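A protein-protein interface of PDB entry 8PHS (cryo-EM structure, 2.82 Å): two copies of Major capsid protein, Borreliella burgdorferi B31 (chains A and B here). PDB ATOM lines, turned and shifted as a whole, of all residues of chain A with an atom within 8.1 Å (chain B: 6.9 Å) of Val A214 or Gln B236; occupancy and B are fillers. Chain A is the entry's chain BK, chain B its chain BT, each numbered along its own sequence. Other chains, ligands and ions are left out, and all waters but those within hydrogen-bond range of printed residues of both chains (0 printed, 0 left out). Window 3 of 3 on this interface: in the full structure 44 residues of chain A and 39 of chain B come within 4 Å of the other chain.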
ATOM      1  N   MET A 177      13.442   0.473   8.478  1.00  0.00           N
ATOM      2  CA  MET A 177      14.533   0.632   9.430  1.00  0.00           C
ATOM      3  C   MET A 177      15.683   1.430   8.836  1.00  0.00           C
ATOM      4  O   MET A 177      16.401   2.112   9.569  1.00  0.00           O
ATOM      5  CB  MET A 177      15.024  -0.736   9.906  1.00  0.00           C
ATOM      6  CG  MET A 177      14.400  -1.193  11.214  1.00  0.00           C
ATOM      7  SD  MET A 177      14.743  -0.091  12.602  1.00  0.00           S
ATOM      8  CE  MET A 177      16.505   0.170  12.420  1.00  0.00           C
ATOM      9  N   PRO A 207       8.741  -1.504  22.365  1.00  0.00           N
ATOM     10  CA  PRO A 207       8.833  -2.913  21.937  1.00  0.00           C
ATOM     11  C   PRO A 207       8.833  -3.111  20.430  1.00  0.00           C
ATOM     12  O   PRO A 207       9.554  -3.984  19.928  1.00  0.00           O
ATOM     13  CB  PRO A 207       7.599  -3.545  22.593  1.00  0.00           C
ATOM     14  CG  PRO A 207       7.377  -2.722  23.810  1.00  0.00           C
ATOM     15  CD  PRO A 207       7.713  -1.316  23.405  1.00  0.00           C
ATOM     16  N   ALA A 208       8.041  -2.333  19.689  1.00  0.00           N
ATOM     17  CA  ALA A 208       8.054  -2.453  18.234  1.00  0.00           C
ATOM     18  C   ALA A 208       9.415  -2.077  17.667  1.00  0.00           C
ATOM     19  O   ALA A 208       9.925  -2.737  16.750  1.00  0.00           O
ATOM     20  CB  ALA A 208       6.956  -1.580  17.627  1.00  0.00           C
ATOM     21  N   THR A 209      10.026  -1.020  18.205  1.00  0.00           N
ATOM     22  CA  THR A 209      11.353  -0.626  17.752  1.00  0.00           C
ATOM     23  C   THR A 209      12.382  -1.702  18.073  1.00  0.00           C
ATOM     24  O   THR A 209      13.289  -1.955  17.276  1.00  0.00           O
ATOM     25  CB  THR A 209      11.749   0.710  18.379  1.00  0.00           C
ATOM     26  OG1 THR A 209      10.826   1.723  17.963  1.00  0.00           O
ATOM     27  CG2 THR A 209      13.147   1.113  17.940  1.00  0.00           C
ATOM     28  N   SER A 210      12.260  -2.347  19.236  1.00  0.00           N
ATOM     29  CA  SER A 210      13.172  -3.442  19.565  1.00  0.00           C
ATOM     30  C   SER A 210      13.003  -4.612  18.600  1.00  0.00           C
ATOM     31  O   SER A 210      13.992  -5.223  18.162  1.00  0.00           O
ATOM     32  CB  SER A 210      12.941  -3.894  21.006  1.00  0.00           C
ATOM     33  OG  SER A 210      13.919  -4.835  21.409  1.00  0.00           O
ATOM     34  N   LEU A 211      11.752  -4.940  18.263  1.00  0.00           N
ATOM     35  CA  LEU A 211      11.493  -5.992  17.286  1.00  0.00           C
ATOM     36  C   LEU A 211      12.129  -5.660  15.943  1.00  0.00           C
ATOM     37  O   LEU A 211      12.698  -6.534  15.282  1.00  0.00           O
ATOM     38  CB  LEU A 211       9.988  -6.200  17.120  1.00  0.00           C
ATOM     39  CG  LEU A 211       9.203  -6.839  18.266  1.00  0.00           C
ATOM     40  CD1 LEU A 211       7.751  -7.034  17.867  1.00  0.00           C
ATOM     41  CD2 LEU A 211       9.822  -8.164  18.663  1.00  0.00           C
ATOM     42  N   LYS A 212      12.035  -4.397  15.522  1.00  0.00           N
ATOM     43  CA  LYS A 212      12.669  -3.996  14.269  1.00  0.00           C
ATOM     44  C   LYS A 212      14.189  -4.029  14.378  1.00  0.00           C
ATOM     45  O   LYS A 212      14.881  -4.351  13.405  1.00  0.00           O
ATOM     46  CB  LYS A 212      12.191  -2.605  13.860  1.00  0.00           C
ATOM     47  CG  LYS A 212      10.725  -2.542  13.485  1.00  0.00           C
ATOM     48  CD  LYS A 212      10.353  -1.168  12.963  1.00  0.00           C
ATOM     49  CE  LYS A 212       8.911  -1.134  12.492  1.00  0.00           C
ATOM     50  NZ  LYS A 212       8.512   0.225  12.039  1.00  0.00           N
ATOM     51  N   LEU A 213      14.728  -3.689  15.551  1.00  0.00           N
ATOM     52  CA  LEU A 213      16.176  -3.625  15.720  1.00  0.00           C
ATOM     53  C   LEU A 213      16.811  -5.005  15.657  1.00  0.00           C
ATOM     54  O   LEU A 213      17.907  -5.163  15.108  1.00  0.00           O
ATOM     55  CB  LEU A 213      16.522  -2.944  17.044  1.00  0.00           C
ATOM     56  CG  LEU A 213      16.462  -1.417  17.084  1.00  0.00           C
ATOM     57  CD1 LEU A 213      16.981  -0.905  18.415  1.00  0.00           C
ATOM     58  CD2 LEU A 213      17.250  -0.820  15.933  1.00  0.00           C
ATOM     59  N   VAL A 214      16.148  -6.019  16.213  1.00  0.00           N
ATOM     60  CA  VAL A 214      16.759  -7.347  16.254  1.00  0.00           C
ATOM     61  C   VAL A 214      16.759  -7.995  14.873  1.00  0.00           C
ATOM     62  O   VAL A 214      17.274  -9.104  14.700  1.00  0.00           O
ATOM     63  CB  VAL A 214      16.065  -8.262  17.279  1.00  0.00           C
ATOM     64  CG1 VAL A 214      16.102  -7.628  18.658  1.00  0.00           C
ATOM     65  CG2 VAL A 214      14.644  -8.565  16.843  1.00  0.00           C
ATOM     66  N   LYS A 215      16.189  -7.313  13.884  1.00  0.00           N
ATOM     67  CA  LYS A 215      16.184  -7.813  12.519  1.00  0.00           C
ATOM     68  C   LYS A 215      17.571  -7.685  11.890  1.00  0.00           C
ATOM     69  O   LYS A 215      18.385  -6.866  12.322  1.00  0.00           O
ATOM     70  CB  LYS A 215      15.155  -7.055  11.688  1.00  0.00           C
ATOM     71  CG  LYS A 215      13.720  -7.316  12.103  1.00  0.00           C
ATOM     72  CD  LYS A 215      13.421  -8.804  12.117  1.00  0.00           C
ATOM     73  CE  LYS A 215      12.039  -9.086  12.680  1.00  0.00           C
ATOM     74  NZ  LYS A 215      11.757 -10.546  12.739  1.00  0.00           N
ATOM     75  N   PRO A 216      17.869  -8.497  10.873  1.00  0.00           N
ATOM     76  CA  PRO A 216      19.180  -8.401  10.220  1.00  0.00           C
ATOM     77  C   PRO A 216      19.378  -7.053   9.543  1.00  0.00           C
ATOM     78  O   PRO A 216      18.443  -6.457   9.005  1.00  0.00           O
ATOM     79  CB  PRO A 216      19.152  -9.541   9.195  1.00  0.00           C
ATOM     80  CG  PRO A 216      18.099 -10.475   9.690  1.00  0.00           C
ATOM     81  CD  PRO A 216      17.067  -9.603  10.326  1.00  0.00           C
ATOM     82  N   TYR A 217      20.621  -6.579   9.572  1.00  0.00           N
ATOM     83  CA  TYR A 217      20.951  -5.301   8.958  1.00  0.00           C
ATOM     84  C   TYR A 217      20.933  -5.413   7.440  1.00  0.00           C
ATOM     85  O   TYR A 217      21.431  -6.386   6.866  1.00  0.00           O
ATOM     86  CB  TYR A 217      22.322  -4.822   9.434  1.00  0.00           C
ATOM     87  CG  TYR A 217      22.891  -3.682   8.622  1.00  0.00           C
ATOM     88  CD1 TYR A 217      22.264  -2.444   8.592  1.00  0.00           C
ATOM     89  CD2 TYR A 217      24.056  -3.843   7.883  1.00  0.00           C
ATOM     90  CE1 TYR A 217      22.780  -1.399   7.851  1.00  0.00           C
ATOM     91  CE2 TYR A 217      24.579  -2.804   7.138  1.00  0.00           C
ATOM     92  CZ  TYR A 217      23.937  -1.585   7.126  1.00  0.00           C
ATOM     93  OH  TYR A 217      24.454  -0.547   6.386  1.00  0.00           O
ATOM     94  N   CYS A 227      26.761 -10.990   8.683  1.00  0.00           N
ATOM     95  CA  CYS A 227      25.612 -11.196   9.556  1.00  0.00           C
ATOM     96  C   CYS A 227      25.621 -10.207  10.715  1.00  0.00           C
ATOM     97  O   CYS A 227      26.078 -10.525  11.813  1.00  0.00           O
ATOM     98  CB  CYS A 227      25.596 -12.631  10.088  1.00  0.00           C
ATOM     99  SG  CYS A 227      24.137 -13.045  11.069  1.00  0.00           S
ATOM    100  N   GLU A 228      25.115  -9.004  10.461  1.00  0.00           N
ATOM    101  CA  GLU A 228      25.068  -7.945  11.456  1.00  0.00           C
ATOM    102  C   GLU A 228      23.628  -7.501  11.672  1.00  0.00           C
ATOM    103  O   GLU A 228      22.763  -7.680  10.810  1.00  0.00           O
ATOM    104  CB  GLU A 228      25.933  -6.751  11.032  1.00  0.00           C
ATOM    105  CG  GLU A 228      26.450  -5.917  12.189  1.00  0.00           C
ATOM    106  CD  GLU A 228      27.344  -4.783  11.733  1.00  0.00           C
ATOM    107  OE1 GLU A 228      27.549  -4.644  10.510  1.00  0.00           O
ATOM    108  OE2 GLU A 228      27.840  -4.031  12.599  1.00  0.00           O
ATOM    109  N   LYS A 229      23.378  -6.920  12.840  1.00  0.00           N
ATOM    110  CA  LYS A 229      22.049  -6.480  13.232  1.00  0.00           C
ATOM    111  C   LYS A 229      21.985  -4.959  13.307  1.00  0.00           C
ATOM    112  O   LYS A 229      22.995  -4.284  13.539  1.00  0.00           O
ATOM    113  CB  LYS A 229      21.646  -7.081  14.580  1.00  0.00           C
ATOM    114  CG  LYS A 229      21.717  -8.596  14.630  1.00  0.00           C
ATOM    115  CD  LYS A 229      20.906  -9.220  13.508  1.00  0.00           C
ATOM    116  CE  LYS A 229      21.138 -10.718  13.432  1.00  0.00           C
ATOM    117  NZ  LYS A 229      20.444 -11.325  12.263  1.00  0.00           N
ATOM    118  N   TRP A 230      20.774  -4.433  13.107  1.00  0.00           N
ATOM    119  CA  TRP A 230      20.555  -2.995  13.221  1.00  0.00           C
ATOM    120  C   TRP A 230      20.978  -2.484  14.591  1.00  0.00           C
ATOM    121  O   TRP A 230      21.508  -1.373  14.712  1.00  0.00           O
ATOM    122  CB  TRP A 230      19.084  -2.669  12.965  1.00  0.00           C
ATOM    123  CG  TRP A 230      18.686  -2.708  11.523  1.00  0.00           C
ATOM    124  CD1 TRP A 230      17.890  -3.635  10.920  1.00  0.00           C
ATOM    125  CD2 TRP A 230      19.049  -1.767  10.506  1.00  0.00           C
ATOM    126  NE1 TRP A 230      17.742  -3.337   9.588  1.00  0.00           N
ATOM    127  CE2 TRP A 230      18.443  -2.194   9.309  1.00  0.00           C
ATOM    128  CE3 TRP A 230      19.831  -0.609  10.491  1.00  0.00           C
ATOM    129  CZ2 TRP A 230      18.596  -1.504   8.109  1.00  0.00           C
ATOM    130  CZ3 TRP A 230      19.979   0.074   9.299  1.00  0.00           C
ATOM    131  CH2 TRP A 230      19.365  -0.375   8.125  1.00  0.00           C
ATOM    132  N   GLU A 231      20.751  -3.283  15.636  1.00  0.00           N
ATOM    133  CA  GLU A 231      21.179  -2.895  16.974  1.00  0.00           C
ATOM    134  C   GLU A 231      22.695  -2.759  17.053  1.00  0.00           C
ATOM    135  O   GLU A 231      23.209  -1.803  17.646  1.00  0.00           O
ATOM    136  CB  GLU A 231      20.674  -3.913  17.996  1.00  0.00           C
ATOM    137  CG  GLU A 231      21.406  -3.883  19.325  1.00  0.00           C
ATOM    138  CD  GLU A 231      20.977  -5.004  20.248  1.00  0.00           C
ATOM    139  OE1 GLU A 231      20.056  -5.762  19.877  1.00  0.00           O
ATOM    140  OE2 GLU A 231      21.561  -5.130  21.345  1.00  0.00           O
ATOM    141  N   ASP A 232      23.427  -3.704  16.457  1.00  0.00           N
ATOM    142  CA  ASP A 232      24.883  -3.616  16.454  1.00  0.00           C
ATOM    143  C   ASP A 232      25.361  -2.393  15.682  1.00  0.00           C
ATOM    144  O   ASP A 232      26.297  -1.704  16.109  1.00  0.00           O
ATOM    145  CB  ASP A 232      25.482  -4.892  15.863  1.00  0.00           C
ATOM    146  CG  ASP A 232      25.139  -6.126  16.672  1.00  0.00           C
ATOM    147  OD1 ASP A 232      24.629  -5.975  17.802  1.00  0.00           O
ATOM    148  OD2 ASP A 232      25.379  -7.249  16.180  1.00  0.00           O
ATOM    149  N   GLU B 228      24.343 -18.163  10.179  1.00  0.00           N
ATOM    150  CA  GLU B 228      23.558 -18.037  11.397  1.00  0.00           C
ATOM    151  C   GLU B 228      22.616 -19.228  11.494  1.00  0.00           C
ATOM    152  O   GLU B 228      22.247 -19.829  10.483  1.00  0.00           O
ATOM    153  CB  GLU B 228      22.773 -16.717  11.416  1.00  0.00           C
ATOM    154  CG  GLU B 228      22.147 -16.369  12.755  1.00  0.00           C
ATOM    155  CD  GLU B 228      21.198 -15.192  12.660  1.00  0.00           C
ATOM    156  OE1 GLU B 228      20.911 -14.748  11.530  1.00  0.00           O
ATOM    157  OE2 GLU B 228      20.743 -14.708  13.717  1.00  0.00           O
ATOM    158  N   LYS B 229      22.235 -19.567  12.721  1.00  0.00           N
ATOM    159  CA  LYS B 229      21.401 -20.728  12.986  1.00  0.00           C
ATOM    160  C   LYS B 229      20.017 -20.309  13.463  1.00  0.00           C
ATOM    161  O   LYS B 229      19.820 -19.219  14.014  1.00  0.00           O
ATOM    162  CB  LYS B 229      22.053 -21.645  14.028  1.00  0.00           C
ATOM    163  CG  LYS B 229      23.471 -22.064  13.687  1.00  0.00           C
ATOM    164  CD  LYS B 229      23.555 -22.626  12.279  1.00  0.00           C
ATOM    165  CE  LYS B 229      24.954 -23.131  11.972  1.00  0.00           C
ATOM    166  NZ  LYS B 229      25.033 -23.744  10.618  1.00  0.00           N
ATOM    167  N   TRP B 230      19.052 -21.205  13.240  1.00  0.00           N
ATOM    168  CA  TRP B 230      17.691 -20.967  13.704  1.00  0.00           C
ATOM    169  C   TRP B 230      17.642 -20.778  15.212  1.00  0.00           C
ATOM    170  O   TRP B 230      16.812 -20.012  15.714  1.00  0.00           O
ATOM    171  CB  TRP B 230      16.784 -22.125  13.289  1.00  0.00           C
ATOM    172  CG  TRP B 230      16.507 -22.182  11.821  1.00  0.00           C
ATOM    173  CD1 TRP B 230      17.080 -23.018  10.911  1.00  0.00           C
ATOM    174  CD2 TRP B 230      15.579 -21.371  11.092  1.00  0.00           C
ATOM    175  NE1 TRP B 230      16.570 -22.778   9.660  1.00  0.00           N
ATOM    176  CE2 TRP B 230      15.646 -21.772   9.744  1.00  0.00           C
ATOM    177  CE3 TRP B 230      14.699 -20.346  11.448  1.00  0.00           C
ATOM    178  CZ2 TRP B 230      14.867 -21.183   8.751  1.00  0.00           C
ATOM    179  CZ3 TRP B 230      13.927 -19.762  10.460  1.00  0.00           C
ATOM    180  CH2 TRP B 230      14.016 -20.181   9.129  1.00  0.00           C
ATOM    181  N   GLU B 231      18.519 -21.461  15.950  1.00  0.00           N
ATOM    182  CA  GLU B 231      18.592 -21.257  17.392  1.00  0.00           C
ATOM    183  C   GLU B 231      18.999 -19.827  17.725  1.00  0.00           C
ATOM    184  O   GLU B 231      18.411 -19.195  18.612  1.00  0.00           O
ATOM    185  CB  GLU B 231      19.569 -22.258  18.007  1.00  0.00           C
ATOM    186  CG  GLU B 231      19.879 -22.018  19.470  1.00  0.00           C
ATOM    187  CD  GLU B 231      20.700 -23.137  20.078  1.00  0.00           C
ATOM    188  OE1 GLU B 231      20.922 -24.154  19.389  1.00  0.00           O
ATOM    189  OE2 GLU B 231      21.124 -23.000  21.244  1.00  0.00           O
ATOM    190  N   ASP B 232      19.997 -19.294  17.015  1.00  0.00           N
ATOM    191  CA  ASP B 232      20.403 -17.908  17.225  1.00  0.00           C
ATOM    192  C   ASP B 232      19.277 -16.943  16.877  1.00  0.00           C
ATOM    193  O   ASP B 232      19.043 -15.962  17.596  1.00  0.00           O
ATOM    194  CB  ASP B 232      21.649 -17.595  16.396  1.00  0.00           C
ATOM    195  CG  ASP B 232      22.830 -18.468  16.764  1.00  0.00           C
ATOM    196  OD1 ASP B 232      22.735 -19.212  17.763  1.00  0.00           O
ATOM    197  OD2 ASP B 232      23.855 -18.412  16.053  1.00  0.00           O
ATOM    198  N   VAL B 233      18.572 -17.204  15.775  1.00  0.00           N
ATOM    199  CA  VAL B 233      17.467 -16.332  15.381  1.00  0.00           C
ATOM    200  C   VAL B 233      16.374 -16.343  16.444  1.00  0.00           C
ATOM    201  O   VAL B 233      15.830 -15.292  16.808  1.00  0.00           O
ATOM    202  CB  VAL B 233      16.921 -16.749  14.002  1.00  0.00           C
ATOM    203  CG1 VAL B 233      15.814 -15.810  13.568  1.00  0.00           C
ATOM    204  CG2 VAL B 233      18.036 -16.761  12.975  1.00  0.00           C
ATOM    205  N   LEU B 234      16.038 -17.528  16.958  1.00  0.00           N
ATOM    206  CA  LEU B 234      15.022 -17.633  17.999  1.00  0.00           C
ATOM    207  C   LEU B 234      15.450 -16.907  19.269  1.00  0.00           C
ATOM    208  O   LEU B 234      14.641 -16.217  19.904  1.00  0.00           O
ATOM    209  CB  LEU B 234      14.734 -19.105  18.293  1.00  0.00           C
ATOM    210  CG  LEU B 234      13.800 -19.409  19.463  1.00  0.00           C
ATOM    211  CD1 LEU B 234      12.359 -19.148  19.072  1.00  0.00           C
ATOM    212  CD2 LEU B 234      13.981 -20.844  19.929  1.00  0.00           C
ATOM    213  N   ILE B 235      16.720 -17.053  19.655  1.00  0.00           N
ATOM    214  CA  ILE B 235      17.210 -16.379  20.855  1.00  0.00           C
ATOM    215  C   ILE B 235      17.121 -14.869  20.691  1.00  0.00           C
ATOM    216  O   ILE B 235      16.698 -14.156  21.609  1.00  0.00           O
ATOM    217  CB  ILE B 235      18.645 -16.836  21.179  1.00  0.00           C
ATOM    218  CG1 ILE B 235      18.643 -18.282  21.672  1.00  0.00           C
ATOM    219  CG2 ILE B 235      19.272 -15.929  22.223  1.00  0.00           C
ATOM    220  CD1 ILE B 235      20.013 -18.801  22.044  1.00  0.00           C
ATOM    221  N   GLN B 236      17.507 -14.354  19.520  1.00  0.00           N
ATOM    222  CA  GLN B 236      17.408 -12.915  19.286  1.00  0.00           C
ATOM    223  C   GLN B 236      15.958 -12.445  19.311  1.00  0.00           C
ATOM    224  O   GLN B 236      15.648 -11.385  19.868  1.00  0.00           O
ATOM    225  CB  GLN B 236      18.066 -12.547  17.958  1.00  0.00           C
ATOM    226  CG  GLN B 236      19.578 -12.657  17.962  1.00  0.00           C
ATOM    227  CD  GLN B 236      20.159 -12.689  16.564  1.00  0.00           C
ATOM    228  OE1 GLN B 236      19.437 -12.541  15.578  1.00  0.00           O
ATOM    229  NE2 GLN B 236      21.468 -12.885  16.470  1.00  0.00           N
ATOM    230  N   THR B 237      15.052 -13.222  18.712  1.00  0.00           N
ATOM    231  CA  THR B 237      13.647 -12.830  18.693  1.00  0.00           C
ATOM    232  C   THR B 237      13.068 -12.776  20.103  1.00  0.00           C
ATOM    233  O   THR B 237      12.291 -11.871  20.428  1.00  0.00           O
ATOM    234  CB  THR B 237      12.845 -13.791  17.818  1.00  0.00           C
ATOM    235  OG1 THR B 237      13.491 -13.925  16.547  1.00  0.00           O
ATOM    236  CG2 THR B 237      11.438 -13.266  17.604  1.00  0.00           C
ATOM    237  N   ILE B 238      13.427 -13.740  20.953  1.00  0.00           N
ATOM    238  CA  ILE B 238      12.941 -13.717  22.331  1.00  0.00           C
ATOM    239  C   ILE B 238      13.594 -12.588  23.125  1.00  0.00           C
ATOM    240  O   ILE B 238      12.960 -11.989  24.009  1.00  0.00           O
ATOM    241  CB  ILE B 238      13.163 -15.088  22.992  1.00  0.00           C
ATOM    242  CG1 ILE B 238      12.401 -16.164  22.220  1.00  0.00           C
ATOM    243  CG2 ILE B 238      12.708 -15.070  24.439  1.00  0.00           C
ATOM    244  CD1 ILE B 238      12.571 -17.547  22.779  1.00  0.00           C
ATOM    245  N   LYS B 239      14.867 -12.292  22.846  1.00  0.00           N
ATOM    246  CA  LYS B 239      15.523 -11.162  23.491  1.00  0.00           C
ATOM    247  C   LYS B 239      14.872  -9.847  23.097  1.00  0.00           C
ATOM    248  O   LYS B 239      14.915  -8.876  23.861  1.00  0.00           O
ATOM    249  CB  LYS B 239      17.010 -11.146  23.138  1.00  0.00           C
ATOM    250  CG  LYS B 239      17.847 -12.113  23.952  1.00  0.00           C
ATOM    251  CD  LYS B 239      19.322 -11.969  23.627  1.00  0.00           C
ATOM    252  CE  LYS B 239      20.171 -12.842  24.532  1.00  0.00           C
ATOM    253  NZ  LYS B 239      20.032 -12.454  25.959  1.00  0.00           N
ATOM    254  N   ALA B 240      14.268  -9.798  21.909  1.00  0.00           N
ATOM    255  CA  ALA B 240      13.554  -8.600  21.486  1.00  0.00           C
ATOM    256  C   ALA B 240      12.371  -8.272  22.387  1.00  0.00           C
ATOM    257  O   ALA B 240      11.926  -7.120  22.405  1.00  0.00           O
ATOM    258  CB  ALA B 240      13.066  -8.760  20.049  1.00  0.00           C
ATOM    259  N   ILE B 241      11.848  -9.248  23.125  1.00  0.00           N
ATOM    260  CA  ILE B 241      10.677  -9.018  23.958  1.00  0.00           C
ATOM    261  C   ILE B 241      10.957  -9.167  25.447  1.00  0.00           C
ATOM    262  O   ILE B 241      10.174  -8.646  26.259  1.00  0.00           O
ATOM    263  CB  ILE B 241       9.507  -9.939  23.550  1.00  0.00           C
ATOM    264  CG1 ILE B 241       9.775 -11.378  23.988  1.00  0.00           C
ATOM    265  CG2 ILE B 241       9.272  -9.872  22.050  1.00  0.00           C
ATOM    266  CD1 ILE B 241       8.567 -12.280  23.879  1.00  0.00           C
ATOM    267  N   ASN B 242      12.025  -9.852  25.859  1.00  0.00           N
ATOM    268  CA  ASN B 242      12.304 -10.006  27.284  1.00  0.00           C
ATOM    269  C   ASN B 242      13.319  -8.986  27.796  1.00  0.00           C
ATOM    270  O   ASN B 242      14.037  -9.259  28.766  1.00  0.00           O
ATOM    271  CB  ASN B 242      12.759 -11.433  27.601  1.00  0.00           C
ATOM    272  CG  ASN B 242      14.197 -11.707  27.199  1.00  0.00           C
ATOM    273  OD1 ASN B 242      14.797 -10.965  26.431  1.00  0.00           O
ATOM    274  ND2 ASN B 242      14.758 -12.782  27.736  1.00  0.00           N
ATOM    275  N   ARG B 244      16.052  -8.089  26.450  1.00  0.00           N
ATOM    276  CA  ARG B 244      17.407  -8.553  26.145  1.00  0.00           C
ATOM    277  C   ARG B 244      18.080  -9.195  27.357  1.00  0.00           C
ATOM    278  O   ARG B 244      19.240  -8.923  27.669  1.00  0.00           O
ATOM    279  CB  ARG B 244      18.262  -7.413  25.585  1.00  0.00           C
ATOM    280  CG  ARG B 244      17.914  -7.037  24.159  1.00  0.00           C
ATOM    281  CD  ARG B 244      18.581  -5.739  23.743  1.00  0.00           C
ATOM    282  NE  ARG B 244      18.124  -5.300  22.430  1.00  0.00           N
ATOM    283  CZ  ARG B 244      16.913  -4.825  22.175  1.00  0.00           C
ATOM    284  NH1 ARG B 244      16.015  -4.669  23.132  1.00  0.00           N
ATOM    285  NH2 ARG B 244      16.598  -4.493  20.927  1.00  0.00           N
ATOM    286  N   VAL B 247      18.063 -16.118  27.825  1.00  0.00           N
ATOM    287  CA  VAL B 247      17.151 -17.080  27.222  1.00  0.00           C
ATOM    288  C   VAL B 247      17.802 -18.450  27.332  1.00  0.00           C
ATOM    289  O   VAL B 247      18.908 -18.657  26.820  1.00  0.00           O
ATOM    290  CB  VAL B 247      16.840 -16.746  25.755  1.00  0.00           C
ATOM    291  CG1 VAL B 247      15.954 -17.817  25.143  1.00  0.00           C
ATOM    292  CG2 VAL B 247      16.183 -15.383  25.651  1.00  0.00           C
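NH1 of Arg B244 lies within hydrogen-bond range of OG of Ser A210 (2.7 Å). O of Ala B240 sits at hydrogen-bond distance from OG of Ser A210, at 3.2 Å. The side-chain amino group (NZ) of Lys A229 lies within salt-bridge range of the side-chain carboxylate (OE1) of Glu B228 (3.5 Å). SG of Cys A227 lies within hydrogen-bond range of OE1 of Glu B228. The side-chain carboxylate (OE1) of Glu A231 is in salt-bridge range of the guanidinium group (NE) of Arg B244.
The side-chain carboxylate of Glu B228 sits close to the side-chain amide oxygen of Gln B236, 3.1 Å away. The backbone carbonyl oxygen (O) of Leu A213 is in hydrogen-bond range of the backbone NH (N) of Glu A231. The backbone carbonyl oxygen of Lys B239 is in hydrogen-bond range of the backbone NH of Arg B244 (2.9 Å). N of Arg B244 lies within hydrogen-bond range of OD1 of Asn B242 (3.1 Å).
Leu A211 touches Ala B240 (CD2 to CB, 3.6 Å). CD2 of Leu A211 touches CG2 of Ile B241 (3.8 Å). Gln B236 touches Val A214. Val A214 touches Ala B240. Val A214 touches Arg B244. Gln B236 touches Lys A229.
Of the printed residues of chain B, Leu A211 touches Ala B240 and Ile B241. Of the printed residues of chain B, Cys A227 touches Glu B228. Printed residues of chain B within 4 Å of Glu A231: Arg B244 (3.2 Å). Gln B236 touches just these residues of chain A: Val A214 and Lys A229. The nearest residue of chain A that does not touch Gln B236 is Cys A227 (6.0 Å). The nearest printed residue of chain B that does not touch Glu A231 is Lys B239 (7.0 Å).
Printed residues of chain B that touch a printed residue of chain A: Glu B228, Gln B236, Ala B240, Ile B241 and Arg B244. Hydrophobic or aromatic side chains of chain B that line the printed part of chain A: Ala B240 and Ile B241. Printed residues of chain A that touch a printed residue of chain B: Ser A210, Leu A211, Val A214, Cys A227, Lys A229 and Glu A231. Hydrophobic or aromatic side chains of chain A that line the printed part of chain B: Leu A211 and Val A214. Among the printed residues, 11 pairs touch across the chains. Among the printed residues, Asp or Glu carboxylates within 4 Å of a Lys or Arg side-chain nitrogen of the other chain: Lys A229 with Glu B228 (3.5 Å) and Glu A231 with Arg B244 (3.2 Å).
Lys A229 touches Glu B228, but with the chains exchanged Glu A228 does not touch Lys B229 (11.2 Å). Positions printed for both chains: 228, 229, 230, 231 and 232. Of the 11 pairs that touch across the chains among the printed residues, none has its exchanged pair printed and touching as well.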
